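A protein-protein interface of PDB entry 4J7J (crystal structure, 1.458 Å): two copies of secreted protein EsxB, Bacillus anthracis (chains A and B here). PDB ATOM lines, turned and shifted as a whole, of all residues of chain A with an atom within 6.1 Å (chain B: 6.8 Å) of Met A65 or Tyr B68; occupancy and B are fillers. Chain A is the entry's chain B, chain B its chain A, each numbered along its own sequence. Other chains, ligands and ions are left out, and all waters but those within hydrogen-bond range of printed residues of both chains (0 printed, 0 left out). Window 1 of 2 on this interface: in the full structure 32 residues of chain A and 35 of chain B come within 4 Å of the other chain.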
ATOM      1  N   ALA A  28      22.643  -1.779  24.624  1.00  0.00           N
ATOM      2  CA  ALA A  28      21.591  -2.298  23.767  1.00  0.00           C
ATOM      3  C   ALA A  28      20.916  -1.167  23.013  1.00  0.00           C
ATOM      4  O   ALA A  28      20.672  -1.269  21.803  1.00  0.00           O
ATOM      5  CB  ALA A  28      20.587  -3.072  24.620  1.00  0.00           C
ATOM      6  N   GLN A  29      20.654  -0.062  23.698  1.00  0.00           N
ATOM      7  CA  GLN A  29      20.025   1.086  23.063  1.00  0.00           C
ATOM      8  C   GLN A  29      20.946   1.686  22.008  1.00  0.00           C
ATOM      9  O   GLN A  29      20.501   2.071  20.924  1.00  0.00           O
ATOM     10  CB  GLN A  29      19.664   2.144  24.109  1.00  0.00           C
ATOM     11  CG  GLN A  29      18.903   3.321  23.519  1.00  0.00           C
ATOM     12  CD  GLN A  29      17.578   2.910  22.893  1.00  0.00           C
ATOM     13  OE1 GLN A  29      16.662   2.467  23.587  1.00  0.00           O
ATOM     14  NE2 GLN A  29      17.469   3.058  21.573  1.00  0.00           N
ATOM     15  N   GLN A  31      23.195   0.115  20.339  1.00  0.00           N
ATOM     16  CA  GLN A  31      23.311  -0.822  19.230  1.00  0.00           C
ATOM     17  C   GLN A  31      22.151  -0.646  18.277  1.00  0.00           C
ATOM     18  O   GLN A  31      22.325  -0.552  17.053  1.00  0.00           O
ATOM     19  CB  GLN A  31      23.312  -2.254  19.746  1.00  0.00           C
ATOM     20  CG  GLN A  31      23.343  -3.263  18.614  1.00  0.00           C
ATOM     21  CD  GLN A  31      23.252  -4.685  19.112  1.00  0.00           C
ATOM     22  OE1 GLN A  31      24.272  -5.356  19.299  1.00  0.00           O
ATOM     23  NE2 GLN A  31      22.036  -5.167  19.296  1.00  0.00           N
ATOM     24  N   ILE A  32      20.949  -0.583  18.824  1.00  0.00           N
ATOM     25  CA  ILE A  32      19.788  -0.438  17.975  1.00  0.00           C
ATOM     26  C   ILE A  32      19.772   0.929  17.282  1.00  0.00           C
ATOM     27  O   ILE A  32      19.316   1.053  16.142  1.00  0.00           O
ATOM     28  CB  ILE A  32      18.487  -0.794  18.717  1.00  0.00           C
ATOM     29  CG1 ILE A  32      17.413  -1.187  17.704  1.00  0.00           C
ATOM     30  CG2 ILE A  32      18.035   0.341  19.613  1.00  0.00           C
ATOM     31  CD1 ILE A  32      16.366  -2.063  18.293  1.00  0.00           C
ATOM     32  N   LEU A  35      22.091   0.553  14.242  1.00  0.00           N
ATOM     33  CA  LEU A  35      21.447  -0.248  13.205  1.00  0.00           C
ATOM     34  C   LEU A  35      20.342   0.550  12.523  1.00  0.00           C
ATOM     35  O   LEU A  35      20.150   0.457  11.300  1.00  0.00           O
ATOM     36  CB  LEU A  35      20.916  -1.564  13.788  1.00  0.00           C
ATOM     37  CG  LEU A  35      21.976  -2.531  14.325  1.00  0.00           C
ATOM     38  CD1 LEU A  35      21.302  -3.691  15.028  1.00  0.00           C
ATOM     39  CD2 LEU A  35      22.896  -3.038  13.222  1.00  0.00           C
ATOM     40  N   GLN A  60      10.190  -4.432  14.154  1.00  0.00           N
ATOM     41  CA  GLN A  60      10.055  -5.636  14.974  1.00  0.00           C
ATOM     42  C   GLN A  60      11.210  -5.800  15.962  1.00  0.00           C
ATOM     43  O   GLN A  60      11.000  -6.148  17.127  1.00  0.00           O
ATOM     44  CB  GLN A  60       9.961  -6.882  14.095  1.00  0.00           C
ATOM     45  CG  GLN A  60       8.638  -7.034  13.369  1.00  0.00           C
ATOM     46  CD  GLN A  60       8.474  -8.416  12.763  1.00  0.00           C
ATOM     47  OE1 GLN A  60       9.232  -8.813  11.875  1.00  0.00           O
ATOM     48  NE2 GLN A  60       7.487  -9.160  13.246  1.00  0.00           N
ATOM     49  N   SER A  61      12.432  -5.534  15.514  1.00  0.00           N
ATOM     50  CA  SER A  61      13.597  -5.659  16.384  1.00  0.00           C
ATOM     51  C   SER A  61      13.563  -4.577  17.458  1.00  0.00           C
ATOM     52  O   SER A  61      13.948  -4.826  18.606  1.00  0.00           O
ATOM     53  CB  SER A  61      14.912  -5.601  15.587  1.00  0.00           C
ATOM     54  OG  SER A  61      15.305  -4.266  15.306  1.00  0.00           O
ATOM     55  N   LYS A  62      13.095  -3.384  17.089  1.00  0.00           N
ATOM     56  CA  LYS A  62      12.921  -2.284  18.045  1.00  0.00           C
ATOM     57  C   LYS A  62      11.918  -2.651  19.125  1.00  0.00           C
ATOM     58  O   LYS A  62      12.112  -2.345  20.306  1.00  0.00           O
ATOM     59  CB  LYS A  62      12.446  -1.013  17.344  1.00  0.00           C
ATOM     60  CG  LYS A  62      13.517  -0.319  16.525  1.00  0.00           C
ATOM     61  CD  LYS A  62      13.028   1.016  15.964  1.00  0.00           C
ATOM     62  CE  LYS A  62      12.781   2.036  17.064  1.00  0.00           C
ATOM     63  NZ  LYS A  62      12.534   3.397  16.513  1.00  0.00           N
ATOM     64  N   GLN A  63      10.843  -3.315  18.735  1.00  0.00           N
ATOM     65  CA  GLN A  63       9.807  -3.675  19.695  1.00  0.00           C
ATOM     66  C   GLN A  63      10.331  -4.700  20.695  1.00  0.00           C
ATOM     67  O   GLN A  63      10.029  -4.617  21.884  1.00  0.00           O
ATOM     68  CB  GLN A  63       8.550  -4.156  18.964  1.00  0.00           C
ATOM     69  CG  GLN A  63       7.766  -2.998  18.352  1.00  0.00           C
ATOM     70  CD  GLN A  63       6.688  -3.439  17.385  1.00  0.00           C
ATOM     71  OE1 GLN A  63       6.665  -4.585  16.933  1.00  0.00           O
ATOM     72  NE2 GLN A  63       5.788  -2.521  17.054  1.00  0.00           N
ATOM     73  N   ALA A  64      11.145  -5.640  20.221  1.00  0.00           N
ATOM     74  CA  ALA A  64      11.785  -6.613  21.106  1.00  0.00           C
ATOM     75  C   ALA A  64      12.723  -5.912  22.083  1.00  0.00           C
ATOM     76  O   ALA A  64      12.796  -6.251  23.265  1.00  0.00           O
ATOM     77  CB  ALA A  64      12.536  -7.663  20.294  1.00  0.00           C
ATOM     78  N   MET A  65      13.437  -4.910  21.594  1.00  0.00           N
ATOM     79  CA  MET A  65      14.384  -4.198  22.438  1.00  0.00           C
ATOM     80  C   MET A  65      13.647  -3.342  23.456  1.00  0.00           C
ATOM     81  O   MET A  65      14.126  -3.140  24.574  1.00  0.00           O
ATOM     82  CB  MET A  65      15.328  -3.334  21.605  1.00  0.00           C
ATOM     83  CG  MET A  65      16.544  -2.881  22.376  1.00  0.00           C
ATOM     84  SD  MET A  65      17.427  -4.327  23.001  1.00  0.00           S
ATOM     85  CE  MET A  65      18.712  -4.472  21.774  1.00  0.00           C
ATOM     86  N   GLN A  66      12.472  -2.859  23.084  1.00  0.00           N
ATOM     87  CA  GLN A  66      11.646  -2.064  23.984  1.00  0.00           C
ATOM     88  C   GLN A  66      11.060  -2.905  25.123  1.00  0.00           C
ATOM     89  O   GLN A  66      10.632  -2.365  26.154  1.00  0.00           O
ATOM     90  CB  GLN A  66      10.569  -1.305  23.204  1.00  0.00           C
ATOM     91  CG  GLN A  66      11.134  -0.070  22.502  1.00  0.00           C
ATOM     92  CD  GLN A  66      10.284   0.410  21.346  1.00  0.00           C
ATOM     93  OE1 GLN A  66       9.157  -0.048  21.152  1.00  0.00           O
ATOM     94  NE2 GLN A  66      10.824   1.339  20.565  1.00  0.00           N
ATOM     95  N   GLN A  67      11.047  -4.225  24.946  1.00  0.00           N
ATOM     96  CA  GLN A  67      10.684  -5.134  26.031  1.00  0.00           C
ATOM     97  C   GLN A  67      11.899  -5.395  26.913  1.00  0.00           C
ATOM     98  O   GLN A  67      11.807  -5.381  28.143  1.00  0.00           O
ATOM     99  CB  GLN A  67      10.171  -6.473  25.491  1.00  0.00           C
ATOM    100  CG  GLN A  67       8.799  -6.434  24.840  1.00  0.00           C
ATOM    101  CD  GLN A  67       8.218  -7.824  24.628  1.00  0.00           C
ATOM    102  OE1 GLN A  67       8.770  -8.819  25.103  1.00  0.00           O
ATOM    103  NE2 GLN A  67       7.097  -7.897  23.923  1.00  0.00           N
ATOM    104  N   TYR A  68      13.035  -5.631  26.270  1.00  0.00           N
ATOM    105  CA  TYR A  68      14.281  -6.016  26.918  1.00  0.00           C
ATOM    106  C   TYR A  68      14.835  -4.958  27.854  1.00  0.00           C
ATOM    107  O   TYR A  68      15.130  -5.244  29.022  1.00  0.00           O
ATOM    108  CB  TYR A  68      15.303  -6.308  25.832  1.00  0.00           C
ATOM    109  CG  TYR A  68      16.663  -6.771  26.294  1.00  0.00           C
ATOM    110  CD1 TYR A  68      16.822  -8.008  26.906  1.00  0.00           C
ATOM    111  CD2 TYR A  68      17.792  -5.996  26.071  1.00  0.00           C
ATOM    112  CE1 TYR A  68      18.068  -8.448  27.308  1.00  0.00           C
ATOM    113  CE2 TYR A  68      19.052  -6.436  26.449  1.00  0.00           C
ATOM    114  CZ  TYR A  68      19.178  -7.667  27.067  1.00  0.00           C
ATOM    115  OH  TYR A  68      20.423  -8.115  27.438  1.00  0.00           O
ATOM    116  N   ILE A  69      14.981  -3.740  27.348  1.00  0.00           N
ATOM    117  CA  ILE A  69      15.619  -2.670  28.102  1.00  0.00           C
ATOM    118  C   ILE A  69      14.967  -2.399  29.467  1.00  0.00           C
ATOM    119  O   ILE A  69      15.673  -2.371  30.477  1.00  0.00           O
ATOM    120  CB  ILE A  69      15.784  -1.387  27.257  1.00  0.00           C
ATOM    121  CG1 ILE A  69      16.877  -1.617  26.217  1.00  0.00           C
ATOM    122  CG2 ILE A  69      16.139  -0.195  28.147  1.00  0.00           C
ATOM    123  CD1 ILE A  69      16.945  -0.562  25.130  1.00  0.00           C
ATOM    124  N   PRO A  70      13.629  -2.231  29.522  1.00  0.00           N
ATOM    125  CA  PRO A  70      13.035  -1.964  30.841  1.00  0.00           C
ATOM    126  C   PRO A  70      13.202  -3.123  31.824  1.00  0.00           C
ATOM    127  O   PRO A  70      13.239  -2.889  33.036  1.00  0.00           O
ATOM    128  CB  PRO A  70      11.551  -1.749  30.527  1.00  0.00           C
ATOM    129  CG  PRO A  70      11.525  -1.314  29.100  1.00  0.00           C
ATOM    130  CD  PRO A  70      12.639  -2.081  28.438  1.00  0.00           C
ATOM    131  N   PHE B  21      24.424  -6.249  11.065  1.00  0.00           N
ATOM    132  CA  PHE B  21      23.322  -6.942  11.716  1.00  0.00           C
ATOM    133  C   PHE B  21      23.768  -8.278  12.299  1.00  0.00           C
ATOM    134  O   PHE B  21      23.388  -8.617  13.426  1.00  0.00           O
ATOM    135  CB  PHE B  21      22.126  -7.084  10.761  1.00  0.00           C
ATOM    136  CG  PHE B  21      21.259  -5.857  10.725  1.00  0.00           C
ATOM    137  CD1 PHE B  21      20.196  -5.723  11.607  1.00  0.00           C
ATOM    138  CD2 PHE B  21      21.568  -4.789   9.882  1.00  0.00           C
ATOM    139  CE1 PHE B  21      19.403  -4.589  11.614  1.00  0.00           C
ATOM    140  CE2 PHE B  21      20.778  -3.643   9.889  1.00  0.00           C
ATOM    141  CZ  PHE B  21      19.699  -3.535  10.754  1.00  0.00           C
ATOM    142  N   ALA B  24      25.883  -7.555  15.334  1.00  0.00           N
ATOM    143  CA  ALA B  24      25.005  -7.129  16.418  1.00  0.00           C
ATOM    144  C   ALA B  24      24.351  -8.327  17.098  1.00  0.00           C
ATOM    145  O   ALA B  24      24.235  -8.355  18.326  1.00  0.00           O
ATOM    146  CB  ALA B  24      23.950  -6.158  15.921  1.00  0.00           C
ATOM    147  N   ALA B  25      23.946  -9.320  16.324  1.00  0.00           N
ATOM    148  CA  ALA B  25      23.349 -10.523  16.879  1.00  0.00           C
ATOM    149  C   ALA B  25      24.339 -11.234  17.804  1.00  0.00           C
ATOM    150  O   ALA B  25      23.979 -11.668  18.915  1.00  0.00           O
ATOM    151  CB  ALA B  25      22.911 -11.438  15.745  1.00  0.00           C
ATOM    152  N   ALA B  28      24.832  -9.300  20.983  1.00  0.00           N
ATOM    153  CA  ALA B  28      23.654  -9.490  21.824  1.00  0.00           C
ATOM    154  C   ALA B  28      23.726 -10.813  22.566  1.00  0.00           C
ATOM    155  O   ALA B  28      23.415 -10.891  23.758  1.00  0.00           O
ATOM    156  CB  ALA B  28      22.380  -9.413  20.989  1.00  0.00           C
ATOM    157  N   GLN B  31      26.215 -10.487  25.327  1.00  0.00           N
ATOM    158  CA  GLN B  31      25.653  -9.725  26.435  1.00  0.00           C
ATOM    159  C   GLN B  31      24.737 -10.577  27.327  1.00  0.00           C
ATOM    160  O   GLN B  31      24.871 -10.584  28.565  1.00  0.00           O
ATOM    161  CB  GLN B  31      24.907  -8.497  25.917  1.00  0.00           C
ATOM    162  CG  GLN B  31      24.336  -7.629  27.036  1.00  0.00           C
ATOM    163  CD  GLN B  31      23.539  -6.451  26.513  1.00  0.00           C
ATOM    164  OE1 GLN B  31      22.317  -6.530  26.375  1.00  0.00           O
ATOM    165  NE2 GLN B  31      24.225  -5.345  26.229  1.00  0.00           N
ATOM    166  N   GLN B  63      14.144 -14.033  27.152  1.00  0.00           N
ATOM    167  CA  GLN B  63      13.109 -14.318  26.162  1.00  0.00           C
ATOM    168  C   GLN B  63      12.957 -13.186  25.142  1.00  0.00           C
ATOM    169  O   GLN B  63      12.780 -13.449  23.955  1.00  0.00           O
ATOM    170  CB  GLN B  63      11.785 -14.649  26.853  1.00  0.00           C
ATOM    171  CG  GLN B  63      11.770 -16.042  27.496  1.00  0.00           C
ATOM    172  CD  GLN B  63      10.615 -16.227  28.455  1.00  0.00           C
ATOM    173  OE1 GLN B  63      10.007 -15.253  28.902  1.00  0.00           O
ATOM    174  NE2 GLN B  63      10.308 -17.479  28.785  1.00  0.00           N
ATOM    175  N   ALA B  64      13.063 -11.931  25.583  1.00  0.00           N
ATOM    176  CA  ALA B  64      12.994 -10.807  24.645  1.00  0.00           C
ATOM    177  C   ALA B  64      14.167 -10.867  23.688  1.00  0.00           C
ATOM    178  O   ALA B  64      14.057 -10.571  22.500  1.00  0.00           O
ATOM    179  CB  ALA B  64      12.994  -9.484  25.387  1.00  0.00           C
ATOM    180  N   MET B  65      15.311 -11.255  24.224  1.00  0.00           N
ATOM    181  CA  MET B  65      16.528 -11.361  23.454  1.00  0.00           C
ATOM    182  C   MET B  65      16.449 -12.487  22.416  1.00  0.00           C
ATOM    183  O   MET B  65      16.989 -12.380  21.292  1.00  0.00           O
ATOM    184  CB  MET B  65      17.676 -11.557  24.443  1.00  0.00           C
ATOM    185  CG  MET B  65      19.043 -11.540  23.868  1.00  0.00           C
ATOM    186  SD  MET B  65      19.441 -10.239  22.683  1.00  0.00           S
ATOM    187  CE  MET B  65      18.606  -8.721  23.181  1.00  0.00           C
ATOM    188  N   GLN B  66      15.766 -13.558  22.791  1.00  0.00           N
ATOM    189  CA  GLN B  66      15.591 -14.691  21.904  1.00  0.00           C
ATOM    190  C   GLN B  66      14.615 -14.375  20.778  1.00  0.00           C
ATOM    191  O   GLN B  66      14.515 -15.120  19.813  1.00  0.00           O
ATOM    192  CB  GLN B  66      15.178 -15.924  22.707  1.00  0.00           C
ATOM    193  CG  GLN B  66      16.354 -16.511  23.478  1.00  0.00           C
ATOM    194  CD  GLN B  66      15.948 -17.588  24.455  1.00  0.00           C
ATOM    195  OE1 GLN B  66      14.777 -17.708  24.810  1.00  0.00           O
ATOM    196  NE2 GLN B  66      16.918 -18.391  24.887  1.00  0.00           N
ATOM    197  N   GLN B  67      13.891 -13.268  20.905  1.00  0.00           N
ATOM    198  CA  GLN B  67      13.105 -12.751  19.787  1.00  0.00           C
ATOM    199  C   GLN B  67      13.954 -11.800  18.937  1.00  0.00           C
ATOM    200  O   GLN B  67      13.933 -11.840  17.706  1.00  0.00           O
ATOM    201  CB  GLN B  67      11.857 -12.022  20.293  1.00  0.00           C
ATOM    202  CG  GLN B  67      10.876 -12.908  21.042  1.00  0.00           C
ATOM    203  CD  GLN B  67      10.272 -13.971  20.156  1.00  0.00           C
ATOM    204  OE1 GLN B  67       9.731 -13.668  19.094  1.00  0.00           O
ATOM    205  NE2 GLN B  67      10.368 -15.228  20.580  1.00  0.00           N
ATOM    206  N   TYR B  68      14.724 -10.949  19.602  1.00  0.00           N
ATOM    207  CA  TYR B  68      15.514  -9.918  18.953  1.00  0.00           C
ATOM    208  C   TYR B  68      16.571 -10.485  18.026  1.00  0.00           C
ATOM    209  O   TYR B  68      16.690 -10.061  16.873  1.00  0.00           O
ATOM    210  CB  TYR B  68      16.193  -9.098  20.044  1.00  0.00           C
ATOM    211  CG  TYR B  68      17.085  -7.981  19.564  1.00  0.00           C
ATOM    212  CD1 TYR B  68      16.558  -6.842  18.956  1.00  0.00           C
ATOM    213  CD2 TYR B  68      18.454  -8.037  19.762  1.00  0.00           C
ATOM    214  CE1 TYR B  68      17.380  -5.805  18.540  1.00  0.00           C
ATOM    215  CE2 TYR B  68      19.284  -6.997  19.362  1.00  0.00           C
ATOM    216  CZ  TYR B  68      18.746  -5.883  18.743  1.00  0.00           C
ATOM    217  OH  TYR B  68      19.568  -4.845  18.367  1.00  0.00           O
ATOM    218  N   ILE B  69      17.348 -11.435  18.527  1.00  0.00           N
ATOM    219  CA  ILE B  69      18.472 -11.965  17.771  1.00  0.00           C
ATOM    220  C   ILE B  69      18.072 -12.556  16.408  1.00  0.00           C
ATOM    221  O   ILE B  69      18.671 -12.193  15.386  1.00  0.00           O
ATOM    222  CB  ILE B  69      19.311 -12.942  18.621  1.00  0.00           C
ATOM    223  CG1 ILE B  69      20.038 -12.169  19.727  1.00  0.00           C
ATOM    224  CG2 ILE B  69      20.299 -13.705  17.749  1.00  0.00           C
ATOM    225  CD1 ILE B  69      20.734 -13.067  20.739  1.00  0.00           C
ATOM    226  N   PRO B  70      17.043 -13.417  16.367  1.00  0.00           N
ATOM    227  CA  PRO B  70      16.678 -13.951  15.050  1.00  0.00           C
ATOM    228  C   PRO B  70      16.139 -12.892  14.107  1.00  0.00           C
ATOM    229  O   PRO B  70      16.275 -13.060  12.889  1.00  0.00           O
ATOM    230  CB  PRO B  70      15.581 -14.977  15.368  1.00  0.00           C
ATOM    231  CG  PRO B  70      15.783 -15.316  16.815  1.00  0.00           C
ATOM    232  CD  PRO B  70      16.324 -14.097  17.467  1.00  0.00           C
ATOM    233  N   ILE B  71      15.535 -11.827  14.627  1.00  0.00           N
ATOM    234  CA  ILE B  71      15.083 -10.746  13.758  1.00  0.00           C
ATOM    235  C   ILE B  71      16.285 -10.085  13.094  1.00  0.00           C
ATOM    236  O   ILE B  71      16.255  -9.818  11.890  1.00  0.00           O
ATOM    237  CB  ILE B  71      14.220  -9.694  14.503  1.00  0.00           C
ATOM    238  CG1 ILE B  71      12.901 -10.313  14.970  1.00  0.00           C
ATOM    239  CG2 ILE B  71      13.919  -8.502  13.598  1.00  0.00           C
ATOM    240  CD1 ILE B  71      12.232  -9.521  16.099  1.00  0.00           C
ATOM    241  N   LEU B  72      17.359  -9.851  13.838  1.00  0.00           N
ATOM    242  CA  LEU B  72      18.569  -9.252  13.257  1.00  0.00           C
ATOM    243  C   LEU B  72      19.181 -10.171  12.212  1.00  0.00           C
ATOM    244  O   LEU B  72      19.638  -9.716  11.161  1.00  0.00           O
ATOM    245  CB  LEU B  72      19.619  -8.957  14.336  1.00  0.00           C
ATOM    246  CG  LEU B  72      19.285  -7.979  15.456  1.00  0.00           C
ATOM    247  CD1 LEU B  72      20.551  -7.694  16.237  1.00  0.00           C
ATOM    248  CD2 LEU B  72      18.674  -6.698  14.914  1.00  0.00           C
ATOM    249  N   GLU B  73      19.186 -11.466  12.490  1.00  0.00           N
ATOM    250  CA  GLU B  73      19.747 -12.440  11.567  1.00  0.00           C
ATOM    251  C   GLU B  73      18.917 -12.494  10.292  1.00  0.00           C
ATOM    252  O   GLU B  73      19.465 -12.628   9.192  1.00  0.00           O
ATOM    253  CB  GLU B  73      19.840 -13.809  12.235  1.00  0.00           C
ATOM    254  CG  GLU B  73      20.935 -13.850  13.306  1.00  0.00           C
ATOM    255  CD  GLU B  73      20.805 -15.042  14.199  1.00  0.00           C
ATOM    256  OE1 GLU B  73      19.688 -15.246  14.708  1.00  0.00           O
ATOM    257  OE2 GLU B  73      21.800 -15.783  14.369  1.00  0.00           O
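OE1 of Gln A31 lies close to O of Ala B24 (3.2 Å).
OE1 of Gln B31 lies within hydrogen-bond range of OH of Tyr A68 (2.7 Å).
The side-chain amide nitrogen (NE2) of Gln A31 sits at hydrogen-bond distance from the side-chain hydroxyl (OH) of Tyr B68 (2.7 Å).
Gln A31 touches Tyr B68, and with the chains exchanged Tyr A68 touches Gln B31.
Ala A64 touches its own counterpart, Ala B64.
Ala A64 touches Tyr B68, and with the chains exchanged Tyr A68 touches Ala B64.
Met A65 touches Tyr B68, but with the chains exchanged Tyr A68 does not touch Met B65 (4.01 Å).
Positions printed for both chains: 28, 31, 63, 64, 65, 66, 67, 68, 69 and 70.
Of the 16 printed residues of chain B, 7 touch a printed residue of chain A.
Of the 16 printed residues of chain A, 8 touch a printed residue of chain B.
Printed residues of chain A that touch a printed residue of chain B: Gln A31, Ile A32, Leu A35, Gln A60, Ser A61, Ala A64, Met A65 and Tyr A68.
Hydrophobic or aromatic side chains of chain A that line the printed part of chain B: Ile A32, Leu A35, Ala A64, Met A65 and Tyr A68.
CZ of Phe B21 touches CB of Leu A35, 3.8 Å away.
Ala B24 touches Leu A35.
CD1 of Leu A35 touches OH of Tyr B68 (3.9 Å).
CD1 of Leu A35 touches CD2 of Leu B72, 3.995 Å away.
Gln A60 touches Ile B71.
Ser A61 touches Tyr B68.
Ser A61 touches Ile B71.
Tyr B68 touches Ala A64.
Met A65 touches Tyr B68 (CE to CZ, 3.3 Å).
Tyr A68 touches Ala B64.
Printed residues of chain A within 4 Å of Tyr B68: Gln A31, Ile A32, Leu A35, Ser A61, Ala A64 and Met A65.
Printed residues of chain B within 4 Å of Ile A32: Tyr B68.
Of the printed residues of chain B, Ala A64 touches Ala B64 (3.9 Å) and Tyr B68 (3.9 Å).
Of the printed residues of chain A, Ile B71 touches Gln A60 and Ser A61.
Of the printed residues of chain B, Ser A61 touches Tyr B68 (3.3 Å), Ile B71 (3.7 Å) and Leu B72 (3.98 Å).
Gln A29 touches none of the printed residues of chain B.
Gln B67 touches none of the printed residues of chain A.
The nearest printed residue of chain B that does not touch Met A65 is Met B65 (4.5 Å).
The nearest printed residue of chain A that does not touch Tyr B68 is Ala A28 (5.1 Å).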
